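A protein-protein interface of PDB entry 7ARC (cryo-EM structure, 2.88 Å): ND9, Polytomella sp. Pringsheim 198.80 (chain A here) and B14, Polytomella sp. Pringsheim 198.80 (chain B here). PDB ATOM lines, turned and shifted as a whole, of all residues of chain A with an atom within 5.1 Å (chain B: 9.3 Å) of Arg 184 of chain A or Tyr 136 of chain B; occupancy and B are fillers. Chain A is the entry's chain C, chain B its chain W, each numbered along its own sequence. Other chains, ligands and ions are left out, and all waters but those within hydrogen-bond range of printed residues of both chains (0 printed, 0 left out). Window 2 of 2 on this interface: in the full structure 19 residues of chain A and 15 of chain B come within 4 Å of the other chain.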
ATOM      1  N   GLU A 182     -25.099  10.486  22.796  1.00  0.00           N
ATOM      2  CA  GLU A 182     -26.184  10.837  23.695  1.00  0.00           C
ATOM      3  C   GLU A 182     -26.669  12.233  23.349  1.00  0.00           C
ATOM      4  O   GLU A 182     -25.934  13.045  22.788  1.00  0.00           O
ATOM      5  CB  GLU A 182     -25.731  10.779  25.156  1.00  0.00           C
ATOM      6  CG  GLU A 182     -26.788  10.308  26.124  1.00  0.00           C
ATOM      7  CD  GLU A 182     -26.271  10.225  27.545  1.00  0.00           C
ATOM      8  OE1 GLU A 182     -25.090  10.562  27.768  1.00  0.00           O
ATOM      9  OE2 GLU A 182     -27.043   9.819  28.438  1.00  0.00           O
ATOM     10  N   VAL A 183     -27.921  12.508  23.695  1.00  0.00           N
ATOM     11  CA  VAL A 183     -28.624  13.711  23.267  1.00  0.00           C
ATOM     12  C   VAL A 183     -28.944  14.545  24.496  1.00  0.00           C
ATOM     13  O   VAL A 183     -29.455  14.023  25.492  1.00  0.00           O
ATOM     14  CB  VAL A 183     -29.894  13.371  22.472  1.00  0.00           C
ATOM     15  CG1 VAL A 183     -30.653  14.617  22.141  1.00  0.00           C
ATOM     16  CG2 VAL A 183     -29.512  12.674  21.186  1.00  0.00           C
ATOM     17  N   ARG A 184     -28.643  15.839  24.422  1.00  0.00           N
ATOM     18  CA  ARG A 184     -28.850  16.754  25.530  1.00  0.00           C
ATOM     19  C   ARG A 184     -29.151  18.138  24.982  1.00  0.00           C
ATOM     20  O   ARG A 184     -28.702  18.496  23.891  1.00  0.00           O
ATOM     21  CB  ARG A 184     -27.603  16.803  26.417  1.00  0.00           C
ATOM     22  CG  ARG A 184     -27.708  17.671  27.640  1.00  0.00           C
ATOM     23  CD  ARG A 184     -26.412  17.621  28.410  1.00  0.00           C
ATOM     24  NE  ARG A 184     -25.312  18.164  27.620  1.00  0.00           N
ATOM     25  CZ  ARG A 184     -25.035  19.456  27.514  1.00  0.00           C
ATOM     26  NH1 ARG A 184     -25.752  20.370  28.145  1.00  0.00           N
ATOM     27  NH2 ARG A 184     -24.012  19.841  26.758  1.00  0.00           N
ATOM     28  N   TYR A 185     -29.915  18.915  25.741  1.00  0.00           N
ATOM     29  CA  TYR A 185     -30.143  20.315  25.416  1.00  0.00           C
ATOM     30  C   TYR A 185     -29.080  21.164  26.099  1.00  0.00           C
ATOM     31  O   TYR A 185     -28.790  20.969  27.284  1.00  0.00           O
ATOM     32  CB  TYR A 185     -31.538  20.761  25.852  1.00  0.00           C
ATOM     33  CG  TYR A 185     -31.752  22.254  25.786  1.00  0.00           C
ATOM     34  CD1 TYR A 185     -32.031  22.878  24.581  1.00  0.00           C
ATOM     35  CD2 TYR A 185     -31.679  23.039  26.925  1.00  0.00           C
ATOM     36  CE1 TYR A 185     -32.227  24.236  24.510  1.00  0.00           C
ATOM     37  CE2 TYR A 185     -31.873  24.401  26.862  1.00  0.00           C
ATOM     38  CZ  TYR A 185     -32.146  24.994  25.652  1.00  0.00           C
ATOM     39  OH  TYR A 185     -32.343  26.352  25.585  1.00  0.00           O
ATOM     40  N   ASP A 186     -28.505  22.103  25.359  1.00  0.00           N
ATOM     41  CA  ASP A 186     -27.515  23.021  25.900  1.00  0.00           C
ATOM     42  C   ASP A 186     -28.150  24.387  26.120  1.00  0.00           C
ATOM     43  O   ASP A 186     -28.917  24.865  25.283  1.00  0.00           O
ATOM     44  CB  ASP A 186     -26.318  23.142  24.958  1.00  0.00           C
ATOM     45  CG  ASP A 186     -25.075  23.643  25.657  1.00  0.00           C
ATOM     46  OD1 ASP A 186     -25.115  23.826  26.891  1.00  0.00           O
ATOM     47  OD2 ASP A 186     -24.055  23.855  24.972  1.00  0.00           O
ATOM     48  N   ARG A 191     -29.986  24.878  21.510  1.00  0.00           N
ATOM     49  CA  ARG A 191     -30.225  23.766  20.606  1.00  0.00           C
ATOM     50  C   ARG A 191     -30.101  22.456  21.366  1.00  0.00           C
ATOM     51  O   ARG A 191     -29.381  22.362  22.362  1.00  0.00           O
ATOM     52  CB  ARG A 191     -29.250  23.788  19.426  1.00  0.00           C
ATOM     53  CG  ARG A 191     -29.470  24.934  18.463  1.00  0.00           C
ATOM     54  CD  ARG A 191     -28.153  25.551  18.068  1.00  0.00           C
ATOM     55  NE  ARG A 191     -27.116  24.540  17.927  1.00  0.00           N
ATOM     56  CZ  ARG A 191     -25.828  24.814  17.790  1.00  0.00           C
ATOM     57  NH1 ARG A 191     -25.386  26.059  17.764  1.00  0.00           N
ATOM     58  NH2 ARG A 191     -24.959  23.813  17.694  1.00  0.00           N
ATOM     59  N   VAL A 192     -30.805  21.442  20.880  1.00  0.00           N
ATOM     60  CA  VAL A 192     -30.645  20.077  21.367  1.00  0.00           C
ATOM     61  C   VAL A 192     -29.517  19.432  20.572  1.00  0.00           C
ATOM     62  O   VAL A 192     -29.568  19.383  19.338  1.00  0.00           O
ATOM     63  CB  VAL A 192     -31.953  19.286  21.232  1.00  0.00           C
ATOM     64  CG1 VAL A 192     -31.698  17.820  21.412  1.00  0.00           C
ATOM     65  CG2 VAL A 192     -32.972  19.770  22.246  1.00  0.00           C
ATOM     66  N   ILE A 193     -28.498  18.931  21.272  1.00  0.00           N
ATOM     67  CA  ILE A 193     -27.254  18.515  20.640  1.00  0.00           C
ATOM     68  C   ILE A 193     -26.928  17.079  21.026  1.00  0.00           C
ATOM     69  O   ILE A 193     -27.403  16.554  22.034  1.00  0.00           O
ATOM     70  CB  ILE A 193     -26.079  19.438  21.018  1.00  0.00           C
ATOM     71  CG1 ILE A 193     -25.834  19.385  22.525  1.00  0.00           C
ATOM     72  CG2 ILE A 193     -26.351  20.859  20.573  1.00  0.00           C
ATOM     73  CD1 ILE A 193     -24.569  20.068  22.962  1.00  0.00           C
ATOM     74  N   SER A 194     -26.104  16.446  20.196  1.00  0.00           N
ATOM     75  CA  SER A 194     -25.635  15.087  20.421  1.00  0.00           C
ATOM     76  C   SER A 194     -24.186  15.110  20.888  1.00  0.00           C
ATOM     77  O   SER A 194     -23.366  15.869  20.365  1.00  0.00           O
ATOM     78  CB  SER A 194     -25.763  14.245  19.152  1.00  0.00           C
ATOM     79  OG  SER A 194     -25.277  12.932  19.364  1.00  0.00           O
ATOM     80  N   GLU A 195     -23.873  14.275  21.870  1.00  0.00           N
ATOM     81  CA  GLU A 195     -22.564  14.242  22.499  1.00  0.00           C
ATOM     82  C   GLU A 195     -22.132  12.797  22.683  1.00  0.00           C
ATOM     83  O   GLU A 195     -22.967  11.887  22.653  1.00  0.00           O
ATOM     84  CB  GLU A 195     -22.586  14.947  23.862  1.00  0.00           C
ATOM     85  CG  GLU A 195     -22.817  16.438  23.797  1.00  0.00           C
ATOM     86  CD  GLU A 195     -22.804  17.076  25.168  1.00  0.00           C
ATOM     87  OE1 GLU A 195     -22.673  16.336  26.163  1.00  0.00           O
ATOM     88  OE2 GLU A 195     -22.918  18.317  25.252  1.00  0.00           O
ATOM     89  N   HIS B  94     -31.259  23.559  12.872  1.00  0.00           N
ATOM     90  CA  HIS B  94     -30.381  23.389  14.021  1.00  0.00           C
ATOM     91  C   HIS B  94     -29.457  22.193  13.848  1.00  0.00           C
ATOM     92  O   HIS B  94     -28.336  22.208  14.361  1.00  0.00           O
ATOM     93  CB  HIS B  94     -31.214  23.255  15.296  1.00  0.00           C
ATOM     94  CG  HIS B  94     -31.822  21.900  15.485  1.00  0.00           C
ATOM     95  ND1 HIS B  94     -32.893  21.455  14.742  1.00  0.00           N
ATOM     96  CD2 HIS B  94     -31.515  20.895  16.339  1.00  0.00           C
ATOM     97  CE1 HIS B  94     -33.217  20.234  15.124  1.00  0.00           C
ATOM     98  NE2 HIS B  94     -32.396  19.870  16.092  1.00  0.00           N
ATOM     99  N   THR B  98     -25.516  22.584  14.143  1.00  0.00           N
ATOM    100  CA  THR B  98     -24.777  21.848  15.158  1.00  0.00           C
ATOM    101  C   THR B  98     -23.678  20.995  14.544  1.00  0.00           C
ATOM    102  O   THR B  98     -22.564  20.938  15.075  1.00  0.00           O
ATOM    103  CB  THR B  98     -25.734  20.975  15.971  1.00  0.00           C
ATOM    104  OG1 THR B  98     -26.715  21.801  16.612  1.00  0.00           O
ATOM    105  CG2 THR B  98     -24.977  20.189  17.030  1.00  0.00           C
ATOM    106  N   ILE B 106     -15.950  27.308  14.916  1.00  0.00           N
ATOM    107  CA  ILE B 106     -15.192  27.213  16.158  1.00  0.00           C
ATOM    108  C   ILE B 106     -13.720  26.994  15.846  1.00  0.00           C
ATOM    109  O   ILE B 106     -12.837  27.607  16.458  1.00  0.00           O
ATOM    110  CB  ILE B 106     -15.761  26.090  17.044  1.00  0.00           C
ATOM    111  CG1 ILE B 106     -16.957  26.595  17.852  1.00  0.00           C
ATOM    112  CG2 ILE B 106     -14.690  25.533  17.970  1.00  0.00           C
ATOM    113  CD1 ILE B 106     -17.821  25.488  18.405  1.00  0.00           C
ATOM    114  N   GLU B 126      -2.812  15.122  30.952  1.00  0.00           N
ATOM    115  CA  GLU B 126      -4.266  15.228  30.883  1.00  0.00           C
ATOM    116  C   GLU B 126      -4.954  14.074  31.607  1.00  0.00           C
ATOM    117  O   GLU B 126      -5.679  14.286  32.584  1.00  0.00           O
ATOM    118  CB  GLU B 126      -4.706  15.299  29.420  1.00  0.00           C
ATOM    119  CG  GLU B 126      -6.198  15.153  29.197  1.00  0.00           C
ATOM    120  CD  GLU B 126      -6.534  14.769  27.769  1.00  0.00           C
ATOM    121  OE1 GLU B 126      -7.152  15.591  27.060  1.00  0.00           O
ATOM    122  OE2 GLU B 126      -6.179  13.648  27.353  1.00  0.00           O
ATOM    123  N   LYS B 127      -4.736  12.842  31.153  1.00  0.00           N
ATOM    124  CA  LYS B 127      -5.462  11.712  31.714  1.00  0.00           C
ATOM    125  C   LYS B 127      -4.619  10.448  31.639  1.00  0.00           C
ATOM    126  O   LYS B 127      -3.670  10.352  30.858  1.00  0.00           O
ATOM    127  CB  LYS B 127      -6.807  11.501  31.014  1.00  0.00           C
ATOM    128  CG  LYS B 127      -6.705  11.124  29.558  1.00  0.00           C
ATOM    129  CD  LYS B 127      -8.084  10.915  28.982  1.00  0.00           C
ATOM    130  CE  LYS B 127      -8.805  12.224  28.800  1.00  0.00           C
ATOM    131  NZ  LYS B 127     -10.109  12.037  28.112  1.00  0.00           N
ATOM    132  N   HIS B 133     -12.251   9.664  25.493  1.00  0.00           N
ATOM    133  CA  HIS B 133     -12.412  10.982  24.901  1.00  0.00           C
ATOM    134  C   HIS B 133     -12.442  12.065  25.976  1.00  0.00           C
ATOM    135  O   HIS B 133     -12.648  11.799  27.162  1.00  0.00           O
ATOM    136  CB  HIS B 133     -13.697  11.044  24.079  1.00  0.00           C
ATOM    137  CG  HIS B 133     -14.943  10.999  24.907  1.00  0.00           C
ATOM    138  ND1 HIS B 133     -15.514   9.819  25.330  1.00  0.00           N
ATOM    139  CD2 HIS B 133     -15.724  11.990  25.397  1.00  0.00           C
ATOM    140  CE1 HIS B 133     -16.595  10.084  26.040  1.00  0.00           C
ATOM    141  NE2 HIS B 133     -16.744  11.394  26.098  1.00  0.00           N
ATOM    142  N   SER B 134     -12.220  13.302  25.541  1.00  0.00           N
ATOM    143  CA  SER B 134     -12.362  14.483  26.381  1.00  0.00           C
ATOM    144  C   SER B 134     -13.443  15.393  25.819  1.00  0.00           C
ATOM    145  O   SER B 134     -13.511  15.611  24.606  1.00  0.00           O
ATOM    146  CB  SER B 134     -11.047  15.258  26.481  1.00  0.00           C
ATOM    147  OG  SER B 134     -10.049  14.492  27.123  1.00  0.00           O
ATOM    148  N   LYS B 135     -14.287  15.922  26.699  1.00  0.00           N
ATOM    149  CA  LYS B 135     -15.338  16.838  26.285  1.00  0.00           C
ATOM    150  C   LYS B 135     -14.970  18.267  26.659  1.00  0.00           C
ATOM    151  O   LYS B 135     -14.327  18.515  27.682  1.00  0.00           O
ATOM    152  CB  LYS B 135     -16.678  16.473  26.923  1.00  0.00           C
ATOM    153  CG  LYS B 135     -17.272  15.172  26.436  1.00  0.00           C
ATOM    154  CD  LYS B 135     -18.611  14.914  27.096  1.00  0.00           C
ATOM    155  CE  LYS B 135     -19.207  13.601  26.633  1.00  0.00           C
ATOM    156  NZ  LYS B 135     -20.516  13.340  27.282  1.00  0.00           N
ATOM    157  N   TYR B 136     -15.393  19.205  25.809  1.00  0.00           N
ATOM    158  CA  TYR B 136     -15.192  20.638  26.034  1.00  0.00           C
ATOM    159  C   TYR B 136     -13.710  20.964  26.188  1.00  0.00           C
ATOM    160  O   TYR B 136     -13.312  21.736  27.062  1.00  0.00           O
ATOM    161  CB  TYR B 136     -15.996  21.132  27.237  1.00  0.00           C
ATOM    162  CG  TYR B 136     -17.375  20.526  27.314  1.00  0.00           C
ATOM    163  CD1 TYR B 136     -18.287  20.702  26.285  1.00  0.00           C
ATOM    164  CD2 TYR B 136     -17.763  19.774  28.410  1.00  0.00           C
ATOM    165  CE1 TYR B 136     -19.545  20.147  26.346  1.00  0.00           C
ATOM    166  CE2 TYR B 136     -19.018  19.215  28.481  1.00  0.00           C
ATOM    167  CZ  TYR B 136     -19.905  19.403  27.446  1.00  0.00           C
ATOM    168  OH  TYR B 136     -21.159  18.847  27.515  1.00  0.00           O
ATOM    169  N   ALA B 137     -12.888  20.366  25.332  1.00  0.00           N
ATOM    170  CA  ALA B 137     -11.444  20.548  25.386  1.00  0.00           C
ATOM    171  C   ALA B 137     -11.053  22.000  25.129  1.00  0.00           C
ATOM    172  O   ALA B 137      -9.997  22.453  25.568  1.00  0.00           O
ATOM    173  CB  ALA B 137     -10.762  19.632  24.386  1.00  0.00           C
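Hydrophobic or aromatic side chains of chain B within 4 Å of the printed part of chain A: His 94 and Tyr 136. Along chain A the printed residues that touch a printed residue of chain B span positions 184 to 195. Among the printed residues, Asp or Glu carboxylates within 4 Å of a Lys or Arg side-chain nitrogen of the other chain: Glu 195 of chain A with Lys 135 of chain B (3.9 Å).
His 94 of chain B touches Arg 191 of chain A (CB to CG, 3.99 Å). Val 192 of chain A touches His 94 of chain B. CG2 of Ile 193 of chain A touches CG2 of Thr 98 of chain B, 3.9 Å away.
Of chain B, only Tyr 136 (3.1 Å) comes within 4 Å of Arg 184 of chain A. Of the printed residues of chain B, Arg 191 of chain A touches His 94 (3.99 Å) and Thr 98 (2.9 Å). Of chain B, only His 94 (3.9 Å) comes within 4 Å of Val 192 of chain A. Of the printed residues of chain B, Glu 195 of chain A touches Lys 135 (3.9 Å) and Tyr 136 (2.9 Å). Of the printed residues of chain A, His 94 of chain B touches Arg 191 (3.99 Å) and Val 192 (3.9 Å). Printed residues of chain A within 4 Å of Thr 98 of chain B: Arg 191 (2.9 Å) and Ile 193 (3.9 Å). Ser 134 of chain B touches none of the printed residues of chain A. Of the printed residues of chain A, Lys 135 of chain B touches Glu 195 (3.9 Å). Of chain A, only Arg 184 and Glu 195 come within 4 Å of Tyr 136 of chain B. Ala 137 of chain B touches none of the printed residues of chain A. The nearest printed residue of chain A that does not touch Tyr 136 of chain B is Ile 193 of chain A (5.8 Å).
OG1 of Thr 98 of chain B sits at hydrogen-bond distance from NH2 of Arg 191 of chain A (2.9 Å). The side-chain hydroxyl (OH) of Tyr 136 of chain B is in hydrogen-bond range of the side-chain carboxylate (OE2) of Glu 195 of chain A (2.9 Å). The side-chain carboxylate (OE1) of Glu 195 of chain A is in salt-bridge range of the side-chain amino group (NZ) of Lys 135 of chain B, at 3.9 Å. The guanidinium group (NH2) of Arg 184 of chain A is in hydrogen-bond range of the side-chain hydroxyl (OH) of Tyr 136 of chain B.
The backbone NH (N) of Glu 182 of chain A is in hydrogen-bond range of the backbone carbonyl oxygen (O) of Glu 195 of chain A, at 2.6 Å. O of Arg 191 of chain A lies within hydrogen-bond range of N of Asp 186 of chain A (3.1 Å). The guanidinium group (NH2) of Arg 184 of chain A is in salt-bridge range of the side-chain carboxylate (OE2) of Glu 195 of chain A (2.4 Å). The backbone carbonyl oxygen of Arg 184 of chain A is in hydrogen-bond range of the backbone NH of Ile 193 of chain A (2.7 Å). The side-chain hydroxyl of Thr 98 of chain B sits at hydrogen-bond distance from the backbone carbonyl oxygen of His 94 of chain B, at 2.8 Å. NH1 of Arg 184 of chain A is in salt-bridge range of OD1 of Asp 186 of chain A (3.7 Å).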
